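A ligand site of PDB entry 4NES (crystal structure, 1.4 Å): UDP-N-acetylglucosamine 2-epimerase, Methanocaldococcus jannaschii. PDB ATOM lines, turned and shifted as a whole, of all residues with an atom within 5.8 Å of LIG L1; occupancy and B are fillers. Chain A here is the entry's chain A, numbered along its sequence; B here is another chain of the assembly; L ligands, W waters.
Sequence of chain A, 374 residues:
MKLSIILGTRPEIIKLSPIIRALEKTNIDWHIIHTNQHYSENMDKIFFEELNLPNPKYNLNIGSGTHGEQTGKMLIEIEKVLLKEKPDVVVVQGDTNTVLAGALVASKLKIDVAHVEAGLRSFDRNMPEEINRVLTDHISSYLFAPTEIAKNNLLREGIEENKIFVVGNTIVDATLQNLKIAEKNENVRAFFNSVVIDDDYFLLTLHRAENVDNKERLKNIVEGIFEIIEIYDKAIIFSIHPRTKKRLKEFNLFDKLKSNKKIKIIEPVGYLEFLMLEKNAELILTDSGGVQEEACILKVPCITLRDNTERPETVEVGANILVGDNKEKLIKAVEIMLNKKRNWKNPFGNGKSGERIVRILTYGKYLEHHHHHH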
ATOM      1  N   THR A   9     -35.219  11.852  30.140  1.00  0.00           N
ATOM      2  CA  THR A   9     -35.139  12.507  28.819  1.00  0.00           C
ATOM      3  C   THR A   9     -36.499  12.713  28.168  1.00  0.00           C
ATOM      4  O   THR A   9     -37.468  12.038  28.524  1.00  0.00           O
ATOM      5  CB  THR A   9     -34.266  11.702  27.826  1.00  0.00           C
ATOM      6  OG1 THR A   9     -34.918  10.459  27.522  1.00  0.00           O
ATOM      7  CG2 THR A   9     -32.872  11.468  28.384  1.00  0.00           C
ATOM      8  N   ARG A  10     -36.538  13.616  27.195  1.00  0.00           N
ATOM      9  CA  ARG A  10     -37.742  13.870  26.395  1.00  0.00           C
ATOM     10  C   ARG A  10     -38.562  12.632  25.977  1.00  0.00           C
ATOM     11  O   ARG A  10     -39.744  12.552  26.315  1.00  0.00           O
ATOM     12  CB  ARG A  10     -37.394  14.733  25.166  1.00  0.00           C
ATOM     13  CG  ARG A  10     -38.525  14.784  24.147  1.00  0.00           C
ATOM     14  CD  ARG A  10     -38.201  15.782  23.036  1.00  0.00           C
ATOM     15  NE  ARG A  10     -37.183  15.303  22.094  1.00  0.00           N
ATOM     16  CZ  ARG A  10     -36.678  16.027  21.111  1.00  0.00           C
ATOM     17  NH1 ARG A  10     -37.045  17.291  20.945  1.00  0.00           N
ATOM     18  NH2 ARG A  10     -35.780  15.487  20.296  1.00  0.00           N
ATOM     19  N   PRO A  11     -37.959  11.670  25.254  1.00  0.00           N
ATOM     20  CA  PRO A  11     -38.795  10.533  24.810  1.00  0.00           C
ATOM     21  C   PRO A  11     -39.338   9.683  25.949  1.00  0.00           C
ATOM     22  O   PRO A  11     -40.436   9.135  25.812  1.00  0.00           O
ATOM     23  CB  PRO A  11     -37.821   9.706  23.960  1.00  0.00           C
ATOM     24  CG  PRO A  11     -36.446  10.089  24.460  1.00  0.00           C
ATOM     25  CD  PRO A  11     -36.563  11.545  24.786  1.00  0.00           C
ATOM     26  N   GLN A  37     -31.259  14.236  33.248  1.00  0.00           N
ATOM     27  CA  GLN A  37     -30.373  14.041  32.112  1.00  0.00           C
ATOM     28  C   GLN A  37     -30.660  15.124  31.080  1.00  0.00           C
ATOM     29  O   GLN A  37     -29.738  15.762  30.560  1.00  0.00           O
ATOM     30  CB  GLN A  37     -30.534  12.647  31.501  1.00  0.00           C
ATOM     31  CG  GLN A  37     -29.570  12.427  30.336  1.00  0.00           C
ATOM     32  CD  GLN A  37     -29.613  11.037  29.743  1.00  0.00           C
ATOM     33  OE1 GLN A  37     -30.072  10.072  30.352  1.00  0.00           O
ATOM     34  NE2 GLN A  37     -29.144  10.942  28.505  1.00  0.00           N
ATOM     35  N   HIS A  38     -31.950  15.324  30.796  1.00  0.00           N
ATOM     36  CA  HIS A  38     -32.417  16.477  30.038  1.00  0.00           C
ATOM     37  C   HIS A  38     -32.925  17.532  31.000  1.00  0.00           C
ATOM     38  O   HIS A  38     -33.561  17.201  32.008  1.00  0.00           O
ATOM     39  CB  HIS A  38     -33.525  16.070  29.064  1.00  0.00           C
ATOM     40  CG  HIS A  38     -33.002  15.361  27.858  1.00  0.00           C
ATOM     41  ND1 HIS A  38     -33.791  15.005  26.801  1.00  0.00           N
ATOM     42  CD2 HIS A  38     -31.747  14.965  27.560  1.00  0.00           C
ATOM     43  CE1 HIS A  38     -33.042  14.424  25.873  1.00  0.00           C
ATOM     44  NE2 HIS A  38     -31.795  14.390  26.316  1.00  0.00           N
ATOM     45  N   TYR A  39     -32.657  18.799  30.685  1.00  0.00           N
ATOM     46  CA  TYR A  39     -32.859  19.910  31.621  1.00  0.00           C
ATOM     47  C   TYR A  39     -33.325  21.175  30.924  1.00  0.00           C
ATOM     48  O   TYR A  39     -33.982  22.015  31.538  1.00  0.00           O
ATOM     49  CB  TYR A  39     -31.569  20.190  32.407  1.00  0.00           C
ATOM     50  CG  TYR A  39     -30.347  20.156  31.527  1.00  0.00           C
ATOM     51  CD1 TYR A  39     -29.922  21.293  30.852  1.00  0.00           C
ATOM     52  CD2 TYR A  39     -29.643  18.984  31.345  1.00  0.00           C
ATOM     53  CE1 TYR A  39     -28.818  21.248  30.024  1.00  0.00           C
ATOM     54  CE2 TYR A  39     -28.534  18.926  30.514  1.00  0.00           C
ATOM     55  CZ  TYR A  39     -28.127  20.065  29.866  1.00  0.00           C
ATOM     56  OH  TYR A  39     -27.032  20.025  29.036  1.00  0.00           O
ATOM     57  N   SER A  40     -32.994  21.329  29.645  1.00  0.00           N
ATOM     58  CA  SER A  40     -33.458  22.491  28.892  1.00  0.00           C
ATOM     59  C   SER A  40     -34.982  22.459  28.891  1.00  0.00           C
ATOM     60  O   SER A  40     -35.581  21.396  28.781  1.00  0.00           O
ATOM     61  CB  SER A  40     -32.932  22.470  27.449  1.00  0.00           C
ATOM     62  OG  SER A  40     -31.521  22.580  27.421  1.00  0.00           O
ATOM     63  N   MET A  43     -36.865  20.546  26.330  1.00  0.00           N
ATOM     64  CA  MET A  43     -36.581  19.117  26.316  1.00  0.00           C
ATOM     65  C   MET A  43     -37.215  18.388  27.482  1.00  0.00           C
ATOM     66  O   MET A  43     -37.132  17.159  27.580  1.00  0.00           O
ATOM     67  CB  MET A  43     -35.064  18.870  26.339  1.00  0.00           C
ATOM     68  CG  MET A  43     -34.340  19.416  25.106  1.00  0.00           C
ATOM     69  SD  MET A  43     -34.917  18.618  23.436  1.00  0.00           S
ATOM     70  CE  MET A  43     -34.118  16.866  23.628  1.00  0.00           C
ATOM     71  N   GLY A  63     -27.579  15.877  34.569  1.00  0.00           N
ATOM     72  CA  GLY A  63     -27.283  16.590  33.331  1.00  0.00           C
ATOM     73  C   GLY A  63     -26.342  15.869  32.400  1.00  0.00           C
ATOM     74  O   GLY A  63     -26.297  14.631  32.362  1.00  0.00           O
ATOM     75  N   SER A  64     -25.568  16.658  31.668  1.00  0.00           N
ATOM     76  CA  SER A  64     -24.742  16.150  30.582  1.00  0.00           C
ATOM     77  C   SER A  64     -23.364  15.695  31.024  1.00  0.00           C
ATOM     78  O   SER A  64     -22.861  16.112  32.071  1.00  0.00           O
ATOM     79  CB  SER A  64     -24.605  17.210  29.493  1.00  0.00           C
ATOM     80  OG  SER A  64     -25.900  17.595  29.030  1.00  0.00           O
ATOM     81  N   GLY A  65     -22.757  14.855  30.211  1.00  0.00           N
ATOM     82  CA  GLY A  65     -21.403  14.397  30.442  1.00  0.00           C
ATOM     83  C   GLY A  65     -21.108  13.227  29.556  1.00  0.00           C
ATOM     84  O   GLY A  65     -21.963  12.764  28.796  1.00  0.00           O
ATOM     85  N   HIS A  67     -20.255   9.185  28.939  1.00  0.00           N
ATOM     86  CA  HIS A  67     -21.070   8.058  29.403  1.00  0.00           C
ATOM     87  C   HIS A  67     -20.702   7.580  30.792  1.00  0.00           C
ATOM     88  O   HIS A  67     -21.560   7.334  31.618  1.00  0.00           O
ATOM     89  CB  HIS A  67     -20.961   6.879  28.435  1.00  0.00           C
ATOM     90  CG  HIS A  67     -21.621   7.127  27.114  1.00  0.00           C
ATOM     91  ND1 HIS A  67     -22.986   7.122  26.956  1.00  0.00           N
ATOM     92  CD2 HIS A  67     -21.092   7.383  25.904  1.00  0.00           C
ATOM     93  CE1 HIS A  67     -23.274   7.378  25.698  1.00  0.00           C
ATOM     94  NE2 HIS A  67     -22.153   7.538  25.029  1.00  0.00           N
ATOM     95  N   GLN A  70     -21.588  10.406  33.431  1.00  0.00           N
ATOM     96  CA  GLN A  70     -23.017  10.587  33.588  1.00  0.00           C
ATOM     97  C   GLN A  70     -23.660   9.355  34.236  1.00  0.00           C
ATOM     98  O   GLN A  70     -24.410   9.476  35.207  1.00  0.00           O
ATOM     99  CB  GLN A  70     -23.628  10.850  32.214  1.00  0.00           C
ATOM    100  CG  GLN A  70     -25.092  11.198  32.217  1.00  0.00           C
ATOM    101  CD  GLN A  70     -25.611  11.335  30.803  1.00  0.00           C
ATOM    102  OE1 GLN A  70     -25.658  10.363  30.059  1.00  0.00           O
ATOM    103  NE2 GLN A  70     -25.975  12.557  30.413  1.00  0.00           N
ATOM    104  N   ASP A  95     -34.127   3.190  26.453  1.00  0.00           N
ATOM    105  CA  ASP A  95     -32.742   2.816  26.212  1.00  0.00           C
ATOM    106  C   ASP A  95     -31.705   3.930  26.452  1.00  0.00           C
ATOM    107  O   ASP A  95     -30.590   3.881  25.910  1.00  0.00           O
ATOM    108  CB  ASP A  95     -32.615   2.286  24.791  1.00  0.00           C
ATOM    109  CG  ASP A  95     -33.133   3.263  23.757  1.00  0.00           C
ATOM    110  OD1 ASP A  95     -33.231   4.467  24.069  1.00  0.00           O
ATOM    111  OD2 ASP A  95     -33.458   2.830  22.642  1.00  0.00           O
ATOM    112  N   THR A  96     -32.030   4.907  27.286  1.00  0.00           N
ATOM    113  CA  THR A  96     -31.102   5.988  27.586  1.00  0.00           C
ATOM    114  C   THR A  96     -30.172   5.561  28.721  1.00  0.00           C
ATOM    115  O   THR A  96     -30.387   4.532  29.352  1.00  0.00           O
ATOM    116  CB  THR A  96     -31.858   7.261  27.991  1.00  0.00           C
ATOM    117  OG1 THR A  96     -32.535   7.018  29.236  1.00  0.00           O
ATOM    118  CG2 THR A  96     -32.881   7.629  26.926  1.00  0.00           C
ATOM    119  N   ASN A  97     -29.152   6.377  28.981  1.00  0.00           N
ATOM    120  CA  ASN A  97     -28.272   6.091  30.126  1.00  0.00           C
ATOM    121  C   ASN A  97     -29.037   6.076  31.446  1.00  0.00           C
ATOM    122  O   ASN A  97     -28.698   5.320  32.355  1.00  0.00           O
ATOM    123  CB  ASN A  97     -27.098   7.066  30.185  1.00  0.00           C
ATOM    124  CG  ASN A  97     -26.058   6.789  29.135  1.00  0.00           C
ATOM    125  OD1 ASN A  97     -26.091   5.771  28.453  1.00  0.00           O
ATOM    126  ND2 ASN A  97     -25.097   7.704  29.014  1.00  0.00           N
ATOM    127  N   THR A  98     -30.081   6.908  31.549  1.00  0.00           N
ATOM    128  CA  THR A  98     -30.922   6.916  32.726  1.00  0.00           C
ATOM    129  C   THR A  98     -31.559   5.543  32.973  1.00  0.00           C
ATOM    130  O   THR A  98     -31.619   5.070  34.104  1.00  0.00           O
ATOM    131  CB  THR A  98     -32.011   7.982  32.601  1.00  0.00           C
ATOM    132  OG1 THR A  98     -31.410   9.275  32.726  1.00  0.00           O
ATOM    133  CG2 THR A  98     -33.072   7.801  33.684  1.00  0.00           C
ATOM    134  N   PRO A 128     -24.779   3.185  21.727  1.00  0.00           N
ATOM    135  CA  PRO A 128     -24.987   3.158  23.178  1.00  0.00           C
ATOM    136  C   PRO A 128     -26.420   2.744  23.563  1.00  0.00           C
ATOM    137  O   PRO A 128     -26.610   2.093  24.604  1.00  0.00           O
ATOM    138  CB  PRO A 128     -24.702   4.599  23.622  1.00  0.00           C
ATOM    139  CG  PRO A 128     -24.805   5.422  22.370  1.00  0.00           C
ATOM    140  CD  PRO A 128     -24.437   4.529  21.230  1.00  0.00           C
ATOM    141  N   GLU A 129     -27.401   3.076  22.736  1.00  0.00           N
ATOM    142  CA  GLU A 129     -28.775   2.692  23.020  1.00  0.00           C
ATOM    143  C   GLU A 129     -28.946   1.187  23.003  1.00  0.00           C
ATOM    144  O   GLU A 129     -29.679   0.648  23.830  1.00  0.00           O
ATOM    145  CB  GLU A 129     -29.749   3.334  22.027  1.00  0.00           C
ATOM    146  CG  GLU A 129     -29.947   4.828  22.214  1.00  0.00           C
ATOM    147  CD  GLU A 129     -28.836   5.670  21.593  1.00  0.00           C
ATOM    148  OE1 GLU A 129     -27.903   5.132  20.946  1.00  0.00           O
ATOM    149  OE2 GLU A 129     -28.893   6.902  21.781  1.00  0.00           O
ATOM    150  N   ASN A 132     -27.486  -0.177  26.176  1.00  0.00           N
ATOM    151  CA  ASN A 132     -28.364   0.107  27.306  1.00  0.00           C
ATOM    152  C   ASN A 132     -29.561  -0.819  27.341  1.00  0.00           C
ATOM    153  O   ASN A 132     -29.940  -1.339  28.397  1.00  0.00           O
ATOM    154  CB  ASN A 132     -28.846   1.557  27.256  1.00  0.00           C
ATOM    155  CG  ASN A 132     -27.759   2.555  27.583  1.00  0.00           C
ATOM    156  OD1 ASN A 132     -26.744   2.199  28.197  1.00  0.00           O
ATOM    157  ND2 ASN A 132     -27.943   3.806  27.171  1.00  0.00           N
ATOM    158  N   HIS A 207     -30.464  13.328  15.470  1.00  0.00           N
ATOM    159  CA  HIS A 207     -29.671  13.455  16.698  1.00  0.00           C
ATOM    160  C   HIS A 207     -28.893  12.216  17.163  1.00  0.00           C
ATOM    161  O   HIS A 207     -28.267  12.262  18.214  1.00  0.00           O
ATOM    162  CB  HIS A 207     -30.528  13.971  17.867  1.00  0.00           C
ATOM    163  CG  HIS A 207     -31.427  12.940  18.486  1.00  0.00           C
ATOM    164  ND1 HIS A 207     -32.678  12.654  18.012  1.00  0.00           N
ATOM    165  CD2 HIS A 207     -31.234  12.143  19.567  1.00  0.00           C
ATOM    166  CE1 HIS A 207     -33.231  11.717  18.753  1.00  0.00           C
ATOM    167  NE2 HIS A 207     -32.371  11.387  19.709  1.00  0.00           N
ATOM    168  N   ARG A 208     -28.949  11.109  16.417  1.00  0.00           N
ATOM    169  CA  ARG A 208     -28.194   9.910  16.837  1.00  0.00           C
ATOM    170  C   ARG A 208     -26.724  10.273  16.965  1.00  0.00           C
ATOM    171  O   ARG A 208     -26.177  10.963  16.101  1.00  0.00           O
ATOM    172  CB  ARG A 208     -28.322   8.773  15.819  1.00  0.00           C
ATOM    173  CG  ARG A 208     -29.715   8.156  15.683  1.00  0.00           C
ATOM    174  CD  ARG A 208     -29.954   6.979  16.628  1.00  0.00           C
ATOM    175  NE  ARG A 208     -29.980   7.334  18.041  1.00  0.00           N
ATOM    176  CZ  ARG A 208     -31.015   7.875  18.671  1.00  0.00           C
ATOM    177  NH1 ARG A 208     -32.133   8.173  17.999  1.00  0.00           N
ATOM    178  NH2 ARG A 208     -30.928   8.138  19.959  1.00  0.00           N
ATOM    179  N   HIS A 241     -32.241  19.205  17.624  1.00  0.00           N
ATOM    180  CA  HIS A 241     -31.871  18.747  18.963  1.00  0.00           C
ATOM    181  C   HIS A 241     -30.642  19.524  19.419  1.00  0.00           C
ATOM    182  O   HIS A 241     -29.786  19.852  18.604  1.00  0.00           O
ATOM    183  CB  HIS A 241     -31.535  17.259  18.854  1.00  0.00           C
ATOM    184  CG  HIS A 241     -31.353  16.554  20.165  1.00  0.00           C
ATOM    185  ND1 HIS A 241     -30.259  16.765  20.984  1.00  0.00           N
ATOM    186  CD2 HIS A 241     -32.085  15.571  20.762  1.00  0.00           C
ATOM    187  CE1 HIS A 241     -30.352  15.979  22.034  1.00  0.00           C
ATOM    188  NE2 HIS A 241     -31.442  15.242  21.929  1.00  0.00           N
ATOM    189  N   PRO A 242     -30.551  19.840  20.721  1.00  0.00           N
ATOM    190  CA  PRO A 242     -29.396  20.630  21.166  1.00  0.00           C
ATOM    191  C   PRO A 242     -28.041  19.960  20.951  1.00  0.00           C
ATOM    192  O   PRO A 242     -27.064  20.672  20.725  1.00  0.00           O
ATOM    193  CB  PRO A 242     -29.675  20.861  22.653  1.00  0.00           C
ATOM    194  CG  PRO A 242     -30.668  19.782  23.040  1.00  0.00           C
ATOM    195  CD  PRO A 242     -31.523  19.609  21.806  1.00  0.00           C
ATOM    196  N   ARG A 243     -27.961  18.629  21.014  1.00  0.00           N
ATOM    197  CA  ARG A 243     -26.714  17.954  20.663  1.00  0.00           C
ATOM    198  C   ARG A 243     -26.329  18.286  19.235  1.00  0.00           C
ATOM    199  O   ARG A 243     -25.172  18.620  18.932  1.00  0.00           O
ATOM    200  CB  ARG A 243     -26.895  16.438  20.783  1.00  0.00           C
ATOM    201  CG  ARG A 243     -25.598  15.657  20.658  1.00  0.00           C
ATOM    202  CD  ARG A 243     -25.867  14.186  20.345  1.00  0.00           C
ATOM    203  NE  ARG A 243     -24.653  13.390  20.522  1.00  0.00           N
ATOM    204  CZ  ARG A 243     -24.385  12.683  21.611  1.00  0.00           C
ATOM    205  NH1 ARG A 243     -25.243  12.628  22.628  1.00  0.00           N
ATOM    206  NH2 ARG A 243     -23.249  12.011  21.689  1.00  0.00           N
ATOM    207  N   LYS A 246     -25.091  21.814  18.584  1.00  0.00           N
ATOM    208  CA  LYS A 246     -23.736  21.969  19.095  1.00  0.00           C
ATOM    209  C   LYS A 246     -22.741  21.373  18.114  1.00  0.00           C
ATOM    210  O   LYS A 246     -21.699  21.978  17.817  1.00  0.00           O
ATOM    211  CB  LYS A 246     -23.607  21.308  20.469  1.00  0.00           C
ATOM    212  CG  LYS A 246     -22.187  21.272  21.018  1.00  0.00           C
ATOM    213  CD  LYS A 246     -22.157  20.675  22.414  1.00  0.00           C
ATOM    214  CE  LYS A 246     -22.455  19.192  22.385  1.00  0.00           C
ATOM    215  NZ  LYS A 246     -22.380  18.619  23.755  1.00  0.00           N
ATOM    216  N   LYS B 108     -18.904   1.750  26.089  1.00  0.00           N
ATOM    217  CA  LYS B 108     -19.412   3.045  25.639  1.00  0.00           C
ATOM    218  C   LYS B 108     -18.347   3.872  24.937  1.00  0.00           C
ATOM    219  O   LYS B 108     -18.663   4.771  24.163  1.00  0.00           O
ATOM    220  CB  LYS B 108     -20.022   3.829  26.805  1.00  0.00           C
ATOM    221  CG  LYS B 108     -21.284   3.209  27.415  1.00  0.00           C
ATOM    222  CD  LYS B 108     -22.472   3.283  26.435  1.00  0.00           C
ATOM    223  CE  LYS B 108     -23.749   2.718  27.047  1.00  0.00           C
ATOM    224  NZ  LYS B 108     -24.313   3.595  28.121  1.00  0.00           N
HETATM  225  C1  LIG L   1     -30.151  11.115  24.819  1.00  0.00           C
HETATM  226  C2  LIG L   1     -30.166   9.616  24.695  1.00  0.00           C
HETATM  227  C3  LIG L   1     -30.764   9.188  23.456  1.00  0.00           C
HETATM  228  C4  LIG L   1     -32.099   9.755  23.221  1.00  0.00           C
HETATM  229  C5  LIG L   1     -32.077  11.257  23.411  1.00  0.00           C
HETATM  230  C6  LIG L   1     -33.430  11.855  23.388  1.00  0.00           C
HETATM  231  C7  LIG L   1     -28.205   8.483  25.910  1.00  0.00           C
HETATM  232  C8  LIG L   1     -26.795   7.997  25.805  1.00  0.00           C
HETATM  233  N1  LIG L   1     -28.773   9.092  24.735  1.00  0.00           N
HETATM  234  O1  LIG L   1     -29.364  11.630  23.803  1.00  0.00           O
HETATM  235  O2  LIG L   1     -30.857   7.753  23.439  1.00  0.00           O
HETATM  236  O3  LIG L   1     -32.564   9.456  21.916  1.00  0.00           O
HETATM  237  O4  LIG L   1     -31.517  11.595  24.676  1.00  0.00           O
HETATM  238  O5  LIG L   1     -33.481  13.140  22.881  1.00  0.00           O
HETATM  239  O6  LIG L   1     -28.848   8.359  26.955  1.00  0.00           O
HETATM  240  N2  LIG L   1     -28.321  18.991  25.755  1.00  0.00           N
HETATM  241  C9  LIG L   1     -28.823  20.182  26.070  1.00  0.00           C
HETATM  242  N3  LIG L   1     -29.909  20.270  26.841  1.00  0.00           N
HETATM  243  C10 LIG L   1     -30.508  19.181  27.343  1.00  0.00           C
HETATM  244  C11 LIG L   1     -30.002  17.919  27.037  1.00  0.00           C
HETATM  245  C12 LIG L   1     -28.884  17.840  26.214  1.00  0.00           C
HETATM  246  O7  LIG L   1     -28.324  21.201  25.641  1.00  0.00           O
HETATM  247  O8  LIG L   1     -31.605  19.298  28.134  1.00  0.00           O
HETATM  248  C13 LIG L   1     -27.135  18.863  24.888  1.00  0.00           C
HETATM  249  C14 LIG L   1     -25.837  18.972  25.580  1.00  0.00           C
HETATM  250  O9  LIG L   1     -24.913  19.625  24.749  1.00  0.00           O
HETATM  251  C15 LIG L   1     -25.450  17.599  25.783  1.00  0.00           C
HETATM  252  C16 LIG L   1     -25.920  16.960  24.534  1.00  0.00           C
HETATM  253  O10 LIG L   1     -27.137  17.611  24.194  1.00  0.00           O
HETATM  254  O11 LIG L   1     -24.078  17.406  26.005  1.00  0.00           O
HETATM  255  C17 LIG L   1     -26.173  15.501  24.688  1.00  0.00           C
HETATM  256  O12 LIG L   1     -27.011  15.152  25.772  1.00  0.00           O
HETATM  257  P1  LIG L   1     -27.151  13.671  26.198  1.00  0.00           P
HETATM  258  O13 LIG L   1     -25.811  13.153  26.604  1.00  0.00           O
HETATM  259  O14 LIG L   1     -28.150  13.586  27.309  1.00  0.00           O
HETATM  260  O15 LIG L   1     -27.581  12.821  24.954  1.00  0.00           O
HETATM  261  P2  LIG L   1     -28.732  13.076  23.890  1.00  0.00           P
HETATM  262  O16 LIG L   1     -28.085  13.355  22.571  1.00  0.00           O
HETATM  263  O17 LIG L   1     -29.727  14.097  24.384  1.00  0.00           O
HETATM  264  N1  LG2 L   2     -40.609  15.345  19.837  1.00  0.00           N
HETATM  265  C1  LG2 L   2     -41.186  16.472  20.315  1.00  0.00           C
HETATM  266  N2  LG2 L   2     -40.754  17.675  19.880  1.00  0.00           N
HETATM  267  C2  LG2 L   2     -39.761  17.806  18.970  1.00  0.00           C
HETATM  268  C3  LG2 L   2     -39.151  16.655  18.451  1.00  0.00           C
HETATM  269  C4  LG2 L   2     -39.592  15.417  18.927  1.00  0.00           C
HETATM  270  O1  LG2 L   2     -42.091  16.408  21.145  1.00  0.00           O
HETATM  271  O2  LG2 L   2     -39.359  19.070  18.557  1.00  0.00           O
HETATM  272  C5  LG2 L   2     -40.995  13.998  20.309  1.00  0.00           C
HETATM  273  C6  LG2 L   2     -41.494  13.051  19.350  1.00  0.00           C
HETATM  274  O3  LG2 L   2     -42.844  13.307  19.058  1.00  0.00           O
HETATM  275  C7  LG2 L   2     -41.240  11.752  20.001  1.00  0.00           C
HETATM  276  C8  LG2 L   2     -40.080  12.001  20.837  1.00  0.00           C
HETATM  277  O4  LG2 L   2     -39.806  13.383  20.784  1.00  0.00           O
HETATM  278  O5  LG2 L   2     -42.296  11.303  20.798  1.00  0.00           O
HETATM  279  C9  LG2 L   2     -38.844  11.298  20.382  1.00  0.00           C
HETATM  280  O6  LG2 L   2     -37.721  11.666  21.139  1.00  0.00           O
HETATM  281  P1  LG2 L   2     -36.254  11.725  20.521  1.00  0.00           P
HETATM  282  O7  LG2 L   2     -35.525  12.879  21.159  1.00  0.00           O
HETATM  283  O8  LG2 L   2     -36.347  11.847  19.019  1.00  0.00           O
HETATM  284  O9  LG2 L   2     -35.487  10.418  20.963  1.00  0.00           O
HETATM  285  P2  LG2 L   2     -35.540   8.910  20.533  1.00  0.00           P
HETATM  286  O10 LG2 L   2     -36.982   8.482  20.295  1.00  0.00           O
HETATM  287  O11 LG2 L   2     -34.680   8.726  19.301  1.00  0.00           O
HETATM  288  O12 LG2 L   2     -34.930   8.215  21.717  1.00  0.00           O
HETATM  289  O   HOH W   1     -22.598  19.228  27.484  1.00  0.00           O
HETATM  290  O   HOH W   2     -26.046  22.295  27.586  1.00  0.00           O
HETATM  291  O   HOH W   3     -27.226   9.031  22.299  1.00  0.00           O
HETATM  292  O   HOH W   4     -24.322  11.275  24.896  1.00  0.00           O
HETATM  293  O   HOH W   5     -25.194  22.292  24.387  1.00  0.00           O
HETATM  294  O   HOH W   6     -27.468  15.441  29.119  1.00  0.00           O
HETATM  295  O   HOH W   7     -25.648  10.592  27.302  1.00  0.00           O
HETATM  296  O   HOH W   8     -23.866  14.900  27.316  1.00  0.00           O
HETATM  297  O   HOH W   9     -33.068   6.425  22.358  1.00  0.00           O
HETATM  298  O   HOH W  10     -28.121  11.210  20.797  1.00  0.00           O
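OE2 of Glu 129 sits at hydrogen-bond distance from O2 of LIG L1 (2.7 Å). N of Tyr 39 lies within hydrogen-bond range of O8 of LIG L1, 2.8 Å away. NE2 of His 38 sits at hydrogen-bond distance from O17 of LIG L1, 2.8 Å away. The backbone NH (N) of Asn 97 sits at hydrogen-bond distance from an oxygen (O6) of LIG L1, at 2.9 Å. O3 of LIG L1 sits at hydrogen-bond distance from NH2 of Arg 208, 2.9 Å away. N of Ser 40 is in hydrogen-bond range of O8 of LIG L1 (2.9 Å). The side-chain hydroxyl of Ser 40 is in hydrogen-bond range of a nitrogen (N3) of LIG L1, at 2.9 Å. The side-chain amino group of Lys 246 is in hydrogen-bond range of an oxygen (O9) of LIG L1. O10 of LIG L1 is in hydrogen-bond range of N of Arg 243. NH1 of Arg 243 lies within salt-bridge range of O16 of LIG L1 (2.9 Å). NE2 of His 207 sits at hydrogen-bond distance from O3 of LIG L1 (2.9 Å). The side-chain amide nitrogen (NE2) of Gln 37 lies within hydrogen-bond range of an oxygen (O6) of LIG L1 (3.0 Å). O5 of LIG L1 sits at hydrogen-bond distance from NE2 of His 241 (3.1 Å). O11 of LG2 L2 lies within salt-bridge range of NH1 of Arg 208 (2.9 Å). A ring nitrogen (NE2) of His 207 lies close to an oxygen (O9) of LG2 L2 (3.5 Å). The guanidinium group (NH2) of Arg 10 lies within salt-bridge range of an oxygen (O7) of LG2 L2, 2.8 Å away.
An oxygen (O3) of LIG L1 is in hydrogen-bond range of an oxygen (O12) of LG2 L2.
The side-chain carboxylate of Glu 129 is in salt-bridge range of the guanidinium group of Arg 208, at 3.0 Å. A ring nitrogen (ND1) of His 38 lies within hydrogen-bond range of the backbone NH (N) of Arg 10, 3.1 Å away. The side-chain amide nitrogen (ND2) of Asn 132 sits at hydrogen-bond distance from the side-chain amide oxygen (OD1) of Asn 97. OE1 of Gln 37 is in hydrogen-bond range of OG1 of Thr 98 (2.8 Å). ND2 of Asn 132 lies close to O of Thr 96, 3.4 Å away. N of Thr 98 sits close to OG1 of Thr 96, 3.4 Å away. NH1 of Arg 10 is in hydrogen-bond range of SD of Met 43, at 3.5 Å. The side-chain amide nitrogen (NE2) of Gln 70 is in hydrogen-bond range of the backbone carbonyl oxygen (O) of Gly 63 (2.9 Å).
Water W7 lies within hydrogen-bond range of O13 of LIG L1 (2.7 Å), OE1 of Gln 70 (2.8 Å) and ND2 of Asn 97 (3.4 Å). Water W6 lies within hydrogen-bond range of the side-chain hydroxyl (OG) of Ser 64 (2.7 Å), an oxygen (O14) of LIG L1 (2.7 Å), the backbone carbonyl oxygen (O) of Gln 37 (2.7 Å) and the side-chain amide nitrogen (NE2) of Gln 70 (3.5 Å). Water W8 lies within hydrogen-bond range of an oxygen (O13) of LIG L1 (2.7 Å) and the backbone NH of Gly 65 (3.1 Å). Water W10 lies within hydrogen-bond range of an oxygen (O16) of LIG L1 (2.8 Å) and the backbone carbonyl oxygen of His 207 (2.8 Å). Water W4 bridges the guanidinium group (NH1) of Arg 243 and an oxygen (O13) of LIG L1. Water W2 lies within hydrogen-bond range of the side-chain hydroxyl (OH) of Tyr 39 (2.9 Å) and an oxygen (O7) of LIG L1 (3.2 Å).
CG2 of Thr 9 touches O4 of LIG L1, 3.9 Å away. Pro 11 touches LIG L1. CE of Met 43 touches O5 of LIG L1 (3.9 Å). Ser 64 touches LIG L1. His 67 touches LIG L1 (CE1 to C8, 3.6 Å). Gln 70 touches LIG L1. Thr 96 touches LIG L1. Pro 242 touches LIG L1. Hydrophobic or aromatic side chains within 4 Å of LIG L1: Pro 11, His 38, Tyr 39, Met 43, His 67, His 207, His 241 and Pro 242. The nearest printed residue that does not touch LIG L1 is Asp 95 (4.1 Å).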
